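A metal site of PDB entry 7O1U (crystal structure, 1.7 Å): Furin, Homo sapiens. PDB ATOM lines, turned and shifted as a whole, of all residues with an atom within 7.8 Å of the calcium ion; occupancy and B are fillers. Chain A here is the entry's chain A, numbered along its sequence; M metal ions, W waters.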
ATOM      1  N   GLY A 148       8.253  25.345 -20.553  1.00  0.00           N
ATOM      2  CA  GLY A 148       7.555  26.500 -20.041  1.00  0.00           C
ATOM      3  C   GLY A 148       6.106  26.134 -19.794  1.00  0.00           C
ATOM      4  O   GLY A 148       5.744  24.962 -19.723  1.00  0.00           O
ATOM      5  N   PRO A 149       5.249  27.145 -19.670  1.00  0.00           N
ATOM      6  CA  PRO A 149       3.840  26.873 -19.378  1.00  0.00           C
ATOM      7  C   PRO A 149       3.155  26.157 -20.533  1.00  0.00           C
ATOM      8  O   PRO A 149       3.603  26.205 -21.680  1.00  0.00           O
ATOM      9  CB  PRO A 149       3.233  28.274 -19.170  1.00  0.00           C
ATOM     10  CG  PRO A 149       4.228  29.230 -19.744  1.00  0.00           C
ATOM     11  CD  PRO A 149       5.572  28.587 -19.667  1.00  0.00           C
ATOM     12  N   GLU A 150       2.051  25.489 -20.198  1.00  0.00           N
ATOM     13  CA  GLU A 150       1.294  24.760 -21.201  1.00  0.00           C
ATOM     14  C   GLU A 150       0.970  25.662 -22.382  1.00  0.00           C
ATOM     15  O   GLU A 150       0.609  26.833 -22.213  1.00  0.00           O
ATOM     16  CB  GLU A 150      -0.003  24.206 -20.598  1.00  0.00           C
ATOM     17  CG  GLU A 150       0.196  23.102 -19.567  1.00  0.00           C
ATOM     18  CD  GLU A 150       1.015  21.940 -20.086  1.00  0.00           C
ATOM     19  OE1 GLU A 150       0.859  21.569 -21.276  1.00  0.00           O
ATOM     20  OE2 GLU A 150       1.825  21.393 -19.308  1.00  0.00           O
ATOM     21  N   ASP A 151       1.106  25.099 -23.586  1.00  0.00           N
ATOM     22  CA  ASP A 151       0.792  25.808 -24.821  1.00  0.00           C
ATOM     23  C   ASP A 151      -0.662  25.593 -25.213  1.00  0.00           C
ATOM     24  O   ASP A 151      -0.971  25.230 -26.350  1.00  0.00           O
ATOM     25  CB  ASP A 151       1.727  25.332 -25.941  1.00  0.00           C
ATOM     26  CG  ASP A 151       3.118  25.922 -25.836  1.00  0.00           C
ATOM     27  OD1 ASP A 151       3.252  27.029 -25.270  1.00  0.00           O
ATOM     28  OD2 ASP A 151       4.074  25.283 -26.337  1.00  0.00           O
ATOM     29  N   ASP A 152      -1.573  25.780 -24.258  1.00  0.00           N
ATOM     30  CA  ASP A 152      -2.993  25.587 -24.505  1.00  0.00           C
ATOM     31  C   ASP A 152      -3.698  26.859 -24.958  1.00  0.00           C
ATOM     32  O   ASP A 152      -4.901  26.816 -25.232  1.00  0.00           O
ATOM     33  CB  ASP A 152      -3.686  25.022 -23.254  1.00  0.00           C
ATOM     34  CG  ASP A 152      -3.469  25.865 -22.015  1.00  0.00           C
ATOM     35  OD1 ASP A 152      -2.909  26.980 -22.112  1.00  0.00           O
ATOM     36  OD2 ASP A 152      -3.869  25.401 -20.923  1.00  0.00           O
ATOM     37  N   GLY A 153      -2.981  27.978 -25.080  1.00  0.00           N
ATOM     38  CA  GLY A 153      -3.593  29.220 -25.490  1.00  0.00           C
ATOM     39  C   GLY A 153      -4.486  29.859 -24.448  1.00  0.00           C
ATOM     40  O   GLY A 153      -5.260  30.755 -24.785  1.00  0.00           O
ATOM     41  N   LYS A 154      -4.399  29.414 -23.200  1.00  0.00           N
ATOM     42  CA  LYS A 154      -5.172  30.060 -22.146  1.00  0.00           C
ATOM     43  C   LYS A 154      -4.364  30.293 -20.880  1.00  0.00           C
ATOM     44  O   LYS A 154      -4.919  30.847 -19.925  1.00  0.00           O
ATOM     45  CB  LYS A 154      -6.427  29.241 -21.821  1.00  0.00           C
ATOM     46  CG  LYS A 154      -6.220  27.781 -21.506  1.00  0.00           C
ATOM     47  CD  LYS A 154      -7.566  27.040 -21.571  1.00  0.00           C
ATOM     48  CE  LYS A 154      -7.395  25.546 -21.316  1.00  0.00           C
ATOM     49  N   THR A 155      -3.089  29.941 -20.850  1.00  0.00           N
ATOM     50  CA  THR A 155      -2.253  30.070 -19.671  1.00  0.00           C
ATOM     51  C   THR A 155      -1.423  31.352 -19.741  1.00  0.00           C
ATOM     52  O   THR A 155      -0.925  31.721 -20.815  1.00  0.00           O
ATOM     53  CB  THR A 155      -1.342  28.841 -19.553  1.00  0.00           C
ATOM     54  OG1 THR A 155      -2.159  27.656 -19.452  1.00  0.00           O
ATOM     55  CG2 THR A 155      -0.448  28.911 -18.319  1.00  0.00           C
ATOM     56  N   ALA A 185      13.164  28.441 -26.840  1.00  0.00           N
ATOM     57  CA  ALA A 185      12.150  28.313 -27.872  1.00  0.00           C
ATOM     58  C   ALA A 185      10.912  29.116 -27.504  1.00  0.00           C
ATOM     59  O   ALA A 185      10.494  29.119 -26.343  1.00  0.00           O
ATOM     60  CB  ALA A 185      11.775  26.842 -28.062  1.00  0.00           C
ATOM     61  N   SER A 186      10.305  29.766 -28.495  1.00  0.00           N
ATOM     62  CA  SER A 186       9.191  30.661 -28.194  1.00  0.00           C
ATOM     63  C   SER A 186       7.862  29.948 -27.966  1.00  0.00           C
ATOM     64  O   SER A 186       6.902  30.611 -27.555  1.00  0.00           O
ATOM     65  CB  SER A 186       9.032  31.686 -29.316  1.00  0.00           C
ATOM     66  OG  SER A 186       8.784  31.059 -30.562  1.00  0.00           O
ATOM     67  N   GLY A 187       7.762  28.652 -28.233  1.00  0.00           N
ATOM     68  CA  GLY A 187       6.561  27.890 -27.930  1.00  0.00           C
ATOM     69  C   GLY A 187       6.069  27.076 -29.118  1.00  0.00           C
ATOM     70  O   GLY A 187       6.508  27.252 -30.262  1.00  0.00           O
ATOM     71  N   ASN A 188       5.112  26.189 -28.820  1.00  0.00           N
ATOM     72  CA  ASN A 188       4.523  25.323 -29.842  1.00  0.00           C
ATOM     73  C   ASN A 188       2.999  25.390 -29.868  1.00  0.00           C
ATOM     74  O   ASN A 188       2.343  24.449 -30.328  1.00  0.00           O
ATOM     75  CB  ASN A 188       4.970  23.878 -29.645  1.00  0.00           C
ATOM     76  CG  ASN A 188       6.321  23.610 -30.226  1.00  0.00           C
ATOM     77  OD1 ASN A 188       6.518  23.742 -31.430  1.00  0.00           O
ATOM     78  ND2 ASN A 188       7.277  23.236 -29.385  1.00  0.00           N
ATOM     79  N   GLY A 189       2.436  26.505 -29.415  1.00  0.00           N
ATOM     80  CA  GLY A 189       0.991  26.618 -29.261  1.00  0.00           C
ATOM     81  C   GLY A 189       0.207  27.195 -30.414  1.00  0.00           C
ATOM     82  O   GLY A 189      -0.917  27.665 -30.242  1.00  0.00           O
ATOM     83  N   GLY A 190       0.775  27.129 -31.626  1.00  0.00           N
ATOM     84  CA  GLY A 190       0.142  27.760 -32.769  1.00  0.00           C
ATOM     85  C   GLY A 190      -1.260  27.265 -33.065  1.00  0.00           C
ATOM     86  O   GLY A 190      -2.139  28.050 -33.417  1.00  0.00           O
ATOM     87  N   HIS A 193      -3.797  28.967 -31.093  1.00  0.00           N
ATOM     88  CA  HIS A 193      -3.758  30.426 -31.235  1.00  0.00           C
ATOM     89  C   HIS A 193      -3.099  31.077 -30.030  1.00  0.00           C
ATOM     90  O   HIS A 193      -3.496  32.156 -29.579  1.00  0.00           O
ATOM     91  CB  HIS A 193      -5.167  30.991 -31.458  1.00  0.00           C
ATOM     92  CG  HIS A 193      -5.879  30.332 -32.599  1.00  0.00           C
ATOM     93  ND1 HIS A 193      -5.611  30.631 -33.911  1.00  0.00           N
ATOM     94  CD2 HIS A 193      -6.819  29.353 -32.617  1.00  0.00           C
ATOM     95  CE1 HIS A 193      -6.364  29.882 -34.693  1.00  0.00           C
ATOM     96  NE2 HIS A 193      -7.105  29.094 -33.933  1.00  0.00           N
ATOM     97  N   ASP A 194      -2.062  30.425 -29.508  1.00  0.00           N
ATOM     98  CA  ASP A 194      -1.333  30.961 -28.377  1.00  0.00           C
ATOM     99  C   ASP A 194      -0.506  32.169 -28.810  1.00  0.00           C
ATOM    100  O   ASP A 194      -0.135  32.316 -29.982  1.00  0.00           O
ATOM    101  CB  ASP A 194      -0.459  29.870 -27.765  1.00  0.00           C
ATOM    102  CG  ASP A 194      -0.083  30.151 -26.316  1.00  0.00           C
ATOM    103  OD1 ASP A 194      -0.462  31.202 -25.762  1.00  0.00           O
ATOM    104  OD2 ASP A 194       0.606  29.279 -25.730  1.00  0.00           O
ATOM    105  N   SER A 195      -0.205  33.031 -27.850  1.00  0.00           N
ATOM    106  CA  SER A 195       0.462  34.319 -28.059  1.00  0.00           C
ATOM    107  C   SER A 195       1.597  34.358 -27.044  1.00  0.00           C
ATOM    108  O   SER A 195       1.339  34.370 -25.838  1.00  0.00           O
ATOM    109  CB  SER A 195      -0.532  35.471 -27.860  1.00  0.00           C
ATOM    110  OG  SER A 195      -0.057  36.729 -28.290  1.00  0.00           O
ATOM    111  N   CYS A 196       2.853  34.325 -27.505  1.00  0.00           N
ATOM    112  CA  CYS A 196       3.908  33.836 -26.623  1.00  0.00           C
ATOM    113  C   CYS A 196       4.414  34.857 -25.603  1.00  0.00           C
ATOM    114  O   CYS A 196       5.221  34.473 -24.747  1.00  0.00           O
ATOM    115  CB  CYS A 196       5.095  33.260 -27.420  1.00  0.00           C
ATOM    116  SG  CYS A 196       5.619  34.034 -29.003  1.00  0.00           S
ATOM    117  N   ASN A 197       3.971  36.121 -25.613  1.00  0.00           N
ATOM    118  CA  ASN A 197       4.343  36.967 -24.483  1.00  0.00           C
ATOM    119  C   ASN A 197       3.654  36.515 -23.188  1.00  0.00           C
ATOM    120  O   ASN A 197       4.028  36.994 -22.110  1.00  0.00           O
ATOM    121  CB  ASN A 197       4.031  38.446 -24.732  1.00  0.00           C
ATOM    122  CG  ASN A 197       4.934  39.082 -25.782  1.00  0.00           C
ATOM    123  OD1 ASN A 197       5.993  38.572 -26.146  1.00  0.00           O
ATOM    124  ND2 ASN A 197       4.504  40.237 -26.283  1.00  0.00           N
ATOM    125  N   CYS A 198       2.661  35.622 -23.273  1.00  0.00           N
ATOM    126  CA  CYS A 198       2.011  35.033 -22.114  1.00  0.00           C
ATOM    127  C   CYS A 198       2.849  33.927 -21.471  1.00  0.00           C
ATOM    128  O   CYS A 198       2.408  33.330 -20.492  1.00  0.00           O
ATOM    129  CB  CYS A 198       0.640  34.465 -22.491  1.00  0.00           C
ATOM    130  SG  CYS A 198      -0.545  35.733 -22.972  1.00  0.00           S
ATOM    131  N   ASP A 199       4.022  33.656 -22.034  1.00  0.00           N
ATOM    132  CA  ASP A 199       4.998  32.693 -21.530  1.00  0.00           C
ATOM    133  C   ASP A 199       6.171  33.495 -20.974  1.00  0.00           C
ATOM    134  O   ASP A 199       6.950  34.071 -21.733  1.00  0.00           O
ATOM    135  CB  ASP A 199       5.381  31.742 -22.675  1.00  0.00           C
ATOM    136  CG  ASP A 199       6.624  30.894 -22.400  1.00  0.00           C
ATOM    137  OD1 ASP A 199       7.350  31.095 -21.407  1.00  0.00           O
ATOM    138  OD2 ASP A 199       6.893  30.014 -23.254  1.00  0.00           O
ATOM    139  N   THR A 202      10.007  32.740 -22.286  1.00  0.00           N
ATOM    140  CA  THR A 202      10.435  33.330 -23.556  1.00  0.00           C
ATOM    141  C   THR A 202      10.276  34.850 -23.543  1.00  0.00           C
ATOM    142  O   THR A 202      11.053  35.554 -24.190  1.00  0.00           O
ATOM    143  CB  THR A 202       9.675  32.660 -24.711  1.00  0.00           C
ATOM    144  OG1 THR A 202      10.321  32.983 -25.959  1.00  0.00           O
ATOM    145  CG2 THR A 202       8.201  33.060 -24.803  1.00  0.00           C
ATOM    146  N   TYR A 222       2.723  25.232 -35.846  1.00  0.00           N
ATOM    147  CA  TYR A 222       2.892  25.241 -34.387  1.00  0.00           C
ATOM    148  C   TYR A 222       3.429  26.567 -33.840  1.00  0.00           C
ATOM    149  O   TYR A 222       3.500  26.737 -32.625  1.00  0.00           O
ATOM    150  CB  TYR A 222       3.845  24.094 -33.970  1.00  0.00           C
ATOM    151  CG  TYR A 222       5.127  24.057 -34.774  1.00  0.00           C
ATOM    152  CD1 TYR A 222       6.167  24.929 -34.484  1.00  0.00           C
ATOM    153  CD2 TYR A 222       5.286  23.187 -35.848  1.00  0.00           C
ATOM    154  CE1 TYR A 222       7.321  24.939 -35.219  1.00  0.00           C
ATOM    155  CE2 TYR A 222       6.442  23.179 -36.590  1.00  0.00           C
ATOM    156  CZ  TYR A 222       7.459  24.059 -36.274  1.00  0.00           C
ATOM    157  OH  TYR A 222       8.632  24.087 -36.994  1.00  0.00           O
ATOM    158  N   GLU A 224       4.108  30.326 -32.504  1.00  0.00           N
ATOM    159  CA  GLU A 224       3.455  31.406 -31.786  1.00  0.00           C
ATOM    160  C   GLU A 224       4.114  32.726 -32.164  1.00  0.00           C
ATOM    161  O   GLU A 224       5.349  32.825 -32.164  1.00  0.00           O
ATOM    162  CB  GLU A 224       3.537  31.212 -30.272  1.00  0.00           C
ATOM    163  CG  GLU A 224       2.869  29.930 -29.772  1.00  0.00           C
ATOM    164  CD  GLU A 224       2.985  29.760 -28.256  1.00  0.00           C
ATOM    165  OE1 GLU A 224       3.226  28.609 -27.812  1.00  0.00           O
ATOM    166  OE2 GLU A 224       2.798  30.759 -27.520  1.00  0.00           O
ATOM    167  N   ARG A 412      -6.696  35.639 -27.837  1.00  0.00           N
ATOM    168  CA  ARG A 412      -6.522  34.200 -27.583  1.00  0.00           C
ATOM    169  C   ARG A 412      -7.893  33.586 -27.371  1.00  0.00           C
ATOM    170  O   ARG A 412      -8.472  33.706 -26.274  1.00  0.00           O
ATOM    171  CB  ARG A 412      -5.617  33.959 -26.380  1.00  0.00           C
ATOM    172  CG  ARG A 412      -4.153  34.322 -26.643  1.00  0.00           C
ATOM    173  CD  ARG A 412      -3.188  33.587 -25.730  1.00  0.00           C
ATOM    174  NE  ARG A 412      -3.507  33.794 -24.320  1.00  0.00           N
ATOM    175  CZ  ARG A 412      -2.950  33.132 -23.312  1.00  0.00           C
ATOM    176  NH1 ARG A 412      -3.327  33.375 -22.064  1.00  0.00           N
ATOM    177  NH2 ARG A 412      -2.016  32.223 -23.539  1.00  0.00           N
HETATM  178 CA    CA M   1       2.975  29.338 -25.513  1.00  0.00          CA
HETATM  179  O   HOH W   1       5.243  30.051 -25.505  1.00  0.00           O
HETATM  180  O   HOH W   2       2.249  31.503 -24.447  1.00  0.00           O
HETATM  181  O   HOH W   3       2.837  28.870 -23.071  1.00  0.00           O
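The calcium ion is bound by the side-chain carboxylate (OD1) of Asp 151, water W1, the side-chain carboxylate (OD2) of Asp 194, the side-chain carboxylate (OE1) of Glu 224, the side-chain carboxylate (OE2) of Glu 224, water W3 and water W2.
The backbone NH of Gly 189 sits close to the side-chain carboxylate of Glu 224 (2.8 Å).
The backbone carbonyl oxygen of Gly 189 sits at hydrogen-bond distance from the backbone NH of Asp 194 (3.1 Å).
The side-chain carboxylate of Asp 151 is in hydrogen-bond range of the backbone NH of Asn 188 (2.8 Å).
The side-chain carboxylate of Asp 194 is in salt-bridge range of the guanidinium group of Arg 412, 2.9 Å away.
The side-chain carboxylate (OE1) of Glu 224 lies close to the backbone NH (N) of Asn 188 (3.2 Å).
Three residues have an atom within 4 Å of the calcium ion: Asp 151, Asp 194 and Glu 224.
Water W1 bridges O of Ser 186 (2.7 Å) and OD2 of Asp 199 (2.8 Å).
Water W2 bridges the side-chain carboxylate (OD1) of Asp 194 and the backbone carbonyl oxygen (O) of Ser 195.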
